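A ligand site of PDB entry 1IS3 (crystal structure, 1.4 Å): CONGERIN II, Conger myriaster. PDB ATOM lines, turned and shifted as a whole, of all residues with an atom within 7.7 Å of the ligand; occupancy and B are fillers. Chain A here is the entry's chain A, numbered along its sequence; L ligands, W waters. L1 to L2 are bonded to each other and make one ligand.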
ATOM      1  N   ARG A  29      -8.572 -20.340  22.699  1.00  0.00           N
ATOM      2  CA  ARG A  29      -9.408 -19.154  22.898  1.00  0.00           C
ATOM      3  C   ARG A  29     -10.873 -19.567  23.027  1.00  0.00           C
ATOM      4  O   ARG A  29     -11.276 -20.642  22.557  1.00  0.00           O
ATOM      5  CB  ARG A  29      -9.255 -18.186  21.712  1.00  0.00           C
ATOM      6  CG  ARG A  29      -9.656 -18.866  20.414  1.00  0.00           C
ATOM      7  CD  ARG A  29      -9.231 -18.226  19.118  1.00  0.00           C
ATOM      8  NE  ARG A  29     -10.019 -17.077  18.790  1.00  0.00           N
ATOM      9  CZ  ARG A  29     -10.585 -16.848  17.594  1.00  0.00           C
ATOM     10  NH1 ARG A  29     -11.263 -15.722  17.461  1.00  0.00           N
ATOM     11  NH2 ARG A  29     -10.556 -17.657  16.543  1.00  0.00           N
ATOM     12  N   SER A  31     -14.998 -17.428  23.138  1.00  0.00           N
ATOM     13  CA  SER A  31     -15.632 -16.109  23.170  1.00  0.00           C
ATOM     14  C   SER A  31     -17.035 -16.131  23.747  1.00  0.00           C
ATOM     15  O   SER A  31     -17.686 -17.177  23.664  1.00  0.00           O
ATOM     16  CB  SER A  31     -15.684 -15.514  21.763  1.00  0.00           C
ATOM     17  OG  SER A  31     -16.382 -16.263  20.781  1.00  0.00           O
ATOM     18  N   ASN A  33     -20.574 -14.026  23.061  1.00  0.00           N
ATOM     19  CA  ASN A  33     -21.093 -13.225  21.941  1.00  0.00           C
ATOM     20  C   ASN A  33     -22.541 -12.799  22.210  1.00  0.00           C
ATOM     21  O   ASN A  33     -23.323 -13.653  22.644  1.00  0.00           O
ATOM     22  CB  ASN A  33     -21.068 -14.057  20.651  1.00  0.00           C
ATOM     23  CG  ASN A  33     -19.672 -14.516  20.325  1.00  0.00           C
ATOM     24  OD1 ASN A  33     -18.894 -13.740  19.806  1.00  0.00           O
ATOM     25  ND2 ASN A  33     -19.250 -15.733  20.677  1.00  0.00           N
ATOM     26  N   HIS A  44     -18.592  -9.096  20.704  1.00  0.00           N
ATOM     27  CA  HIS A  44     -17.812 -10.314  20.696  1.00  0.00           C
ATOM     28  C   HIS A  44     -16.687 -10.133  21.734  1.00  0.00           C
ATOM     29  O   HIS A  44     -15.939  -9.170  21.577  1.00  0.00           O
ATOM     30  CB  HIS A  44     -17.230 -10.534  19.298  1.00  0.00           C
ATOM     31  CG  HIS A  44     -16.154 -11.632  19.166  1.00  0.00           C
ATOM     32  ND1 HIS A  44     -16.308 -12.947  19.155  1.00  0.00           N
ATOM     33  CD2 HIS A  44     -14.793 -11.418  18.911  1.00  0.00           C
ATOM     34  CE1 HIS A  44     -15.155 -13.547  18.908  1.00  0.00           C
ATOM     35  NE2 HIS A  44     -14.247 -12.612  18.768  1.00  0.00           N
ATOM     36  N   MET A  45     -16.500 -10.972  22.755  1.00  0.00           N
ATOM     37  CA  MET A  45     -15.437 -10.812  23.734  1.00  0.00           C
ATOM     38  C   MET A  45     -14.635 -12.113  23.628  1.00  0.00           C
ATOM     39  O   MET A  45     -15.072 -13.199  24.069  1.00  0.00           O
ATOM     40  CB  MET A  45     -16.099 -10.659  25.066  1.00  0.00           C
ATOM     41  CG  MET A  45     -15.076 -10.569  26.144  1.00  0.00           C
ATOM     42  SD  MET A  45     -15.949 -10.506  27.732  1.00  0.00           S
ATOM     43  CE  MET A  45     -14.640  -9.677  28.551  1.00  0.00           C
ATOM     44  N   ASP A  46     -13.458 -12.062  23.018  1.00  0.00           N
ATOM     45  CA  ASP A  46     -12.655 -13.225  22.797  1.00  0.00           C
ATOM     46  C   ASP A  46     -11.552 -13.297  23.849  1.00  0.00           C
ATOM     47  O   ASP A  46     -10.912 -12.293  24.179  1.00  0.00           O
ATOM     48  CB  ASP A  46     -12.097 -13.143  21.390  1.00  0.00           C
ATOM     49  CG  ASP A  46     -11.587 -14.459  20.847  1.00  0.00           C
ATOM     50  OD1 ASP A  46     -12.069 -15.514  21.239  1.00  0.00           O
ATOM     51  OD2 ASP A  46     -10.696 -14.448  20.012  1.00  0.00           O
ATOM     52  N   HIS A  47     -11.350 -14.479  24.413  1.00  0.00           N
ATOM     53  CA  HIS A  47     -10.417 -14.704  25.504  1.00  0.00           C
ATOM     54  C   HIS A  47      -9.300 -15.524  24.892  1.00  0.00           C
ATOM     55  O   HIS A  47      -9.510 -16.710  24.604  1.00  0.00           O
ATOM     56  CB  HIS A  47     -11.067 -15.497  26.666  1.00  0.00           C
ATOM     57  CG  HIS A  47     -12.353 -14.895  27.189  1.00  0.00           C
ATOM     58  ND1 HIS A  47     -13.520 -14.811  26.522  1.00  0.00           N
ATOM     59  CD2 HIS A  47     -12.554 -14.428  28.456  1.00  0.00           C
ATOM     60  CE1 HIS A  47     -14.429 -14.316  27.337  1.00  0.00           C
ATOM     61  NE2 HIS A  47     -13.831 -14.101  28.491  1.00  0.00           N
ATOM     62  N   ARG A  48      -8.140 -14.905  24.646  1.00  0.00           N
ATOM     63  CA  ARG A  48      -7.086 -15.592  23.890  1.00  0.00           C
ATOM     64  C   ARG A  48      -5.944 -16.032  24.779  1.00  0.00           C
ATOM     65  O   ARG A  48      -5.203 -15.193  25.317  1.00  0.00           O
ATOM     66  CB  ARG A  48      -6.556 -14.668  22.810  1.00  0.00           C
ATOM     67  CG  ARG A  48      -7.608 -14.393  21.724  1.00  0.00           C
ATOM     68  CD  ARG A  48      -7.174 -13.321  20.719  1.00  0.00           C
ATOM     69  NE  ARG A  48      -8.258 -13.048  19.754  1.00  0.00           N
ATOM     70  CZ  ARG A  48      -8.138 -12.358  18.613  1.00  0.00           C
ATOM     71  NH1 ARG A  48      -9.192 -12.164  17.803  1.00  0.00           N
ATOM     72  NH2 ARG A  48      -6.964 -11.835  18.302  1.00  0.00           N
ATOM     73  N   TYR A  51      -3.294 -17.423  20.479  1.00  0.00           N
ATOM     74  CA  TYR A  51      -3.924 -17.297  19.184  1.00  0.00           C
ATOM     75  C   TYR A  51      -3.059 -16.372  18.373  1.00  0.00           C
ATOM     76  O   TYR A  51      -3.034 -15.166  18.617  1.00  0.00           O
ATOM     77  CB  TYR A  51      -5.363 -16.712  19.330  1.00  0.00           C
ATOM     78  CG  TYR A  51      -6.068 -16.472  17.995  1.00  0.00           C
ATOM     79  CD1 TYR A  51      -6.399 -17.544  17.164  1.00  0.00           C
ATOM     80  CD2 TYR A  51      -6.381 -15.174  17.607  1.00  0.00           C
ATOM     81  CE1 TYR A  51      -7.050 -17.323  15.948  1.00  0.00           C
ATOM     82  CE2 TYR A  51      -7.041 -14.937  16.400  1.00  0.00           C
ATOM     83  CZ  TYR A  51      -7.371 -16.026  15.575  1.00  0.00           C
ATOM     84  OH  TYR A  51      -8.039 -15.769  14.391  1.00  0.00           O
ATOM     85  N   ALA A  53      -0.169 -14.215  17.467  1.00  0.00           N
ATOM     86  CA  ALA A  53       0.750 -13.561  18.377  1.00  0.00           C
ATOM     87  C   ALA A  53       0.085 -13.181  19.675  1.00  0.00           C
ATOM     88  O   ALA A  53       0.759 -12.607  20.523  1.00  0.00           O
ATOM     89  CB  ALA A  53       1.298 -12.269  17.805  1.00  0.00           C
ATOM     90  N   ASP A  54      -1.215 -13.399  19.864  1.00  0.00           N
ATOM     91  CA  ASP A  54      -1.917 -13.029  21.083  1.00  0.00           C
ATOM     92  C   ASP A  54      -1.866 -14.081  22.163  1.00  0.00           C
ATOM     93  O   ASP A  54      -2.234 -15.248  21.935  1.00  0.00           O
ATOM     94  CB  ASP A  54      -3.374 -12.748  20.744  1.00  0.00           C
ATOM     95  CG  ASP A  54      -3.550 -11.431  20.005  1.00  0.00           C
ATOM     96  OD1 ASP A  54      -2.844 -10.485  20.341  1.00  0.00           O
ATOM     97  OD2 ASP A  54      -4.395 -11.331  19.131  1.00  0.00           O
ATOM     98  N   VAL A  59      -9.894  -9.593  23.450  1.00  0.00           N
ATOM     99  CA  VAL A  59     -10.098  -8.814  22.241  1.00  0.00           C
ATOM    100  C   VAL A  59     -11.615  -8.632  22.094  1.00  0.00           C
ATOM    101  O   VAL A  59     -12.376  -9.624  22.119  1.00  0.00           O
ATOM    102  CB  VAL A  59      -9.494  -9.563  21.027  1.00  0.00           C
ATOM    103  CG1 VAL A  59      -9.792  -8.809  19.714  1.00  0.00           C
ATOM    104  CG2 VAL A  59      -7.969  -9.672  21.208  1.00  0.00           C
ATOM    105  N   LEU A  60     -12.077  -7.389  21.958  1.00  0.00           N
ATOM    106  CA  LEU A  60     -13.490  -7.076  21.795  1.00  0.00           C
ATOM    107  C   LEU A  60     -13.774  -6.472  20.422  1.00  0.00           C
ATOM    108  O   LEU A  60     -12.980  -5.664  19.907  1.00  0.00           O
ATOM    109  CB  LEU A  60     -13.933  -6.100  22.884  1.00  0.00           C
ATOM    110  CG  LEU A  60     -13.872  -6.753  24.267  1.00  0.00           C
ATOM    111  CD1 LEU A  60     -12.534  -6.424  24.916  1.00  0.00           C
ATOM    112  CD2 LEU A  60     -15.030  -6.269  25.094  1.00  0.00           C
ATOM    113  N   ASN A  61     -14.887  -6.867  19.804  1.00  0.00           N
ATOM    114  CA  ASN A  61     -15.235  -6.346  18.490  1.00  0.00           C
ATOM    115  C   ASN A  61     -16.691  -6.598  18.135  1.00  0.00           C
ATOM    116  O   ASN A  61     -17.413  -7.236  18.921  1.00  0.00           O
ATOM    117  CB  ASN A  61     -14.310  -6.990  17.427  1.00  0.00           C
ATOM    118  CG  ASN A  61     -14.045  -6.132  16.182  1.00  0.00           C
ATOM    119  OD1 ASN A  61     -14.718  -5.151  15.913  1.00  0.00           O
ATOM    120  ND2 ASN A  61     -13.097  -6.492  15.349  1.00  0.00           N
ATOM    121  N   SER A  62     -17.191  -6.033  17.038  1.00  0.00           N
ATOM    122  CA  SER A  62     -18.521  -6.305  16.534  1.00  0.00           C
ATOM    123  C   SER A  62     -18.340  -6.880  15.132  1.00  0.00           C
ATOM    124  O   SER A  62     -17.349  -6.593  14.417  1.00  0.00           O
ATOM    125  CB  SER A  62     -19.298  -5.004  16.535  1.00  0.00           C
ATOM    126  OG  SER A  62     -18.616  -4.042  15.733  1.00  0.00           O
ATOM    127  N   LEU A  63     -19.325  -7.671  14.742  1.00  0.00           N
ATOM    128  CA  LEU A  63     -19.375  -8.348  13.473  1.00  0.00           C
ATOM    129  C   LEU A  63     -20.660  -7.929  12.809  1.00  0.00           C
ATOM    130  O   LEU A  63     -21.738  -8.070  13.420  1.00  0.00           O
ATOM    131  CB  LEU A  63     -19.388  -9.870  13.669  1.00  0.00           C
ATOM    132  CG  LEU A  63     -19.501 -10.749  12.441  1.00  0.00           C
ATOM    133  CD1 LEU A  63     -18.293 -10.608  11.546  1.00  0.00           C
ATOM    134  CD2 LEU A  63     -19.558 -12.190  12.887  1.00  0.00           C
ATOM    135  N   TRP A  69     -15.792  -8.008  10.485  1.00  0.00           N
ATOM    136  CA  TRP A  69     -15.324  -7.492  11.750  1.00  0.00           C
ATOM    137  C   TRP A  69     -14.968  -6.020  11.662  1.00  0.00           C
ATOM    138  O   TRP A  69     -14.433  -5.591  10.635  1.00  0.00           O
ATOM    139  CB  TRP A  69     -14.105  -8.338  12.212  1.00  0.00           C
ATOM    140  CG  TRP A  69     -14.501  -9.758  12.642  1.00  0.00           C
ATOM    141  CD1 TRP A  69     -14.243 -10.847  11.848  1.00  0.00           C
ATOM    142  CD2 TRP A  69     -15.204 -10.117  13.787  1.00  0.00           C
ATOM    143  NE1 TRP A  69     -14.761 -11.895  12.470  1.00  0.00           N
ATOM    144  CE2 TRP A  69     -15.341 -11.510  13.623  1.00  0.00           C
ATOM    145  CE3 TRP A  69     -15.737  -9.479  14.927  1.00  0.00           C
ATOM    146  CZ2 TRP A  69     -16.028 -12.255  14.611  1.00  0.00           C
ATOM    147  CZ3 TRP A  69     -16.416 -10.228  15.886  1.00  0.00           C
ATOM    148  CH2 TRP A  69     -16.550 -11.607  15.725  1.00  0.00           C
ATOM    149  N   GLN A  70     -15.283  -5.251  12.696  1.00  0.00           N
ATOM    150  CA  GLN A  70     -15.040  -3.824  12.728  1.00  0.00           C
ATOM    151  C   GLN A  70     -13.726  -3.537  13.467  1.00  0.00           C
ATOM    152  O   GLN A  70     -12.799  -4.355  13.356  1.00  0.00           O
ATOM    153  CB  GLN A  70     -16.270  -3.168  13.382  1.00  0.00           C
ATOM    154  CG  GLN A  70     -17.511  -3.452  12.492  1.00  0.00           C
ATOM    155  CD  GLN A  70     -17.340  -3.086  11.000  1.00  0.00           C
ATOM    156  OE1 GLN A  70     -17.145  -1.918  10.658  1.00  0.00           O
ATOM    157  NE2 GLN A  70     -17.394  -4.037  10.067  1.00  0.00           N
ATOM    158  N   GLN A  71     -13.584  -2.429  14.180  1.00  0.00           N
ATOM    159  CA  GLN A  71     -12.324  -2.082  14.815  1.00  0.00           C
ATOM    160  C   GLN A  71     -12.205  -2.834  16.158  1.00  0.00           C
ATOM    161  O   GLN A  71     -13.065  -2.713  17.037  1.00  0.00           O
ATOM    162  CB  GLN A  71     -12.339  -0.575  14.977  1.00  0.00           C
ATOM    163  CG  GLN A  71     -11.114   0.039  15.608  1.00  0.00           C
ATOM    164  CD  GLN A  71     -11.352   0.902  16.872  1.00  0.00           C
ATOM    165  OE1 GLN A  71     -11.728   2.091  16.837  1.00  0.00           O
ATOM    166  NE2 GLN A  71     -11.085   0.354  18.075  1.00  0.00           N
ATOM    167  N   GLU A  72     -11.143  -3.619  16.343  1.00  0.00           N
ATOM    168  CA  GLU A  72     -10.854  -4.322  17.609  1.00  0.00           C
ATOM    169  C   GLU A  72     -10.456  -3.404  18.748  1.00  0.00           C
ATOM    170  O   GLU A  72      -9.748  -2.401  18.532  1.00  0.00           O
ATOM    171  CB  GLU A  72      -9.677  -5.266  17.565  1.00  0.00           C
ATOM    172  CG  GLU A  72      -9.744  -6.239  16.468  1.00  0.00           C
ATOM    173  CD  GLU A  72      -8.631  -7.257  16.510  1.00  0.00           C
ATOM    174  OE1 GLU A  72      -7.509  -6.988  16.963  1.00  0.00           O
ATOM    175  OE2 GLU A  72      -8.911  -8.343  16.059  1.00  0.00           O
ATOM    176  N   GLU A  73     -10.864  -3.737  19.959  1.00  0.00           N
ATOM    177  CA  GLU A  73     -10.410  -3.076  21.166  1.00  0.00           C
ATOM    178  C   GLU A  73      -9.779  -4.194  21.955  1.00  0.00           C
ATOM    179  O   GLU A  73     -10.225  -5.340  21.877  1.00  0.00           O
ATOM    180  CB  GLU A  73     -11.577  -2.481  21.909  1.00  0.00           C
ATOM    181  CG  GLU A  73     -11.867  -1.178  21.115  1.00  0.00           C
ATOM    182  CD  GLU A  73     -12.860  -0.164  21.666  1.00  0.00           C
ATOM    183  OE1 GLU A  73     -13.413   0.618  20.860  1.00  0.00           O
ATOM    184  OE2 GLU A  73     -13.076  -0.142  22.887  1.00  0.00           O
ATOM    185  N   ARG A  74      -8.657  -3.929  22.604  1.00  0.00           N
ATOM    186  CA  ARG A  74      -7.946  -4.953  23.376  1.00  0.00           C
ATOM    187  C   ARG A  74      -7.760  -4.621  24.840  1.00  0.00           C
ATOM    188  O   ARG A  74      -7.677  -3.442  25.199  1.00  0.00           O
ATOM    189  CB  ARG A  74      -6.577  -5.200  22.766  1.00  0.00           C
ATOM    190  CG  ARG A  74      -6.725  -5.919  21.436  1.00  0.00           C
ATOM    191  CD  ARG A  74      -5.600  -5.672  20.444  1.00  0.00           C
ATOM    192  NE  ARG A  74      -5.755  -6.527  19.267  1.00  0.00           N
ATOM    193  CZ  ARG A  74      -5.272  -7.784  19.296  1.00  0.00           C
ATOM    194  NH1 ARG A  74      -4.647  -8.247  20.380  1.00  0.00           N
ATOM    195  NH2 ARG A  74      -5.410  -8.585  18.235  1.00  0.00           N
HETATM  196  C1  LIG L   1      -5.985  -9.584  14.270  1.00  0.00           C
HETATM  197  C2  LIG L   1      -6.820 -10.720  14.862  1.00  0.00           C
HETATM  198  C3  LIG L   1      -7.910 -11.117  13.870  1.00  0.00           C
HETATM  199  C4  LIG L   1      -7.273 -11.492  12.518  1.00  0.00           C
HETATM  200  C5  LIG L   1      -8.299 -11.777  11.441  1.00  0.00           C
HETATM  201  C6  LIG L   1      -5.409 -10.049  12.926  1.00  0.00           C
HETATM  202  O1  LIG L   1      -4.683  -9.014  12.362  1.00  0.00           O
HETATM  203  O2  LIG L   1      -4.936  -9.236  15.159  1.00  0.00           O
HETATM  204  O3  LIG L   1      -7.400 -10.311  16.082  1.00  0.00           O
HETATM  205  O4  LIG L   1      -8.631 -12.253  14.372  1.00  0.00           O
HETATM  206  O5  LIG L   1      -6.466 -10.386  12.033  1.00  0.00           O
HETATM  207  O6  LIG L   1      -9.184 -10.686  11.268  1.00  0.00           O
HETATM  208  C1  LG2 L   2     -10.020 -12.175  14.360  1.00  0.00           C
HETATM  209  C2  LG2 L   2     -10.584 -13.570  14.624  1.00  0.00           C
HETATM  210  C3  LG2 L   2     -12.087 -13.518  14.785  1.00  0.00           C
HETATM  211  C4  LG2 L   2     -12.478 -12.484  15.846  1.00  0.00           C
HETATM  212  C5  LG2 L   2     -11.856 -11.137  15.479  1.00  0.00           C
HETATM  213  C6  LG2 L   2     -12.162 -10.065  16.489  1.00  0.00           C
HETATM  214  O1  LG2 L   2     -10.248 -14.419  13.550  1.00  0.00           O
HETATM  215  O2  LG2 L   2     -12.578 -14.800  15.159  1.00  0.00           O
HETATM  216  O3  LG2 L   2     -12.032 -12.885  17.133  1.00  0.00           O
HETATM  217  O4  LG2 L   2     -10.422 -11.260  15.395  1.00  0.00           O
HETATM  218  O5  LG2 L   2     -11.629  -8.823  16.069  1.00  0.00           O
HETATM  219  O   HOH W   1      -3.898 -11.631  16.531  1.00  0.00           O
HETATM  220  O   HOH W   2     -10.395 -14.767  10.241  1.00  0.00           O
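The side-chain carboxylate of Glu 72 is in hydrogen-bond range of an oxygen (O3) of LIG L1 (2.5 Å).
O1 of LG2 L2 is in hydrogen-bond range of OH of Tyr 51, 2.7 Å away.
The guanidinium group (NH2) of Arg 48 lies within hydrogen-bond range of an oxygen (O3) of LIG L1, at 2.7 Å.
A ring nitrogen (NE2) of His 44 lies within hydrogen-bond range of an oxygen (O3) of LG2 L2 (2.8 Å).
O2 of LG2 L2 is in hydrogen-bond range of NH1 of Arg 29.
ND2 of Asn 61 lies within hydrogen-bond range of O5 of LG2 L2, 2.8 Å away.
O2 of LIG L1 sits at hydrogen-bond distance from NH2 of Arg 74.
Water W1 bridges OD2 of Asp 54 (2.7 Å) and O2 of LIG L1 (2.9 Å).
Merely in contact with the ligand: Asp 46 and Trp 69.
Nine residues have an atom within 4 Å of the ligand: Arg 29, His 44, Asp 46, Arg 48, Tyr 51, Asn 61, Trp 69, Glu 72 and Arg 74.
The guanidinium group (NE) of Arg 48 is in salt-bridge range of the side-chain carboxylate (OD2) of Asp 46, 2.8 Å away.
The guanidinium group of Arg 48 is in salt-bridge range of the side-chain carboxylate of Asp 54 (2.7 Å).
The backbone NH of His 44 lies within hydrogen-bond range of the backbone carbonyl oxygen of Asn 61, at 2.8 Å.
A ring nitrogen (ND1) of His 44 lies within hydrogen-bond range of the side-chain amide oxygen of Asn 33 (2.8 Å).
The side-chain carboxylate (OD2) of Asp 46 is in salt-bridge range of the guanidinium group (NH1) of Arg 29, 2.9 Å away.
ND2 of Asn 61 lies within hydrogen-bond range of O of Gln 70, 2.9 Å away.
The side-chain amide oxygen (OD1) of Asn 61 sits close to the backbone carbonyl oxygen (O) of Gln 71, at 3.2 Å.
N of Asp 46 is in hydrogen-bond range of O of Val 59 (2.8 Å).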
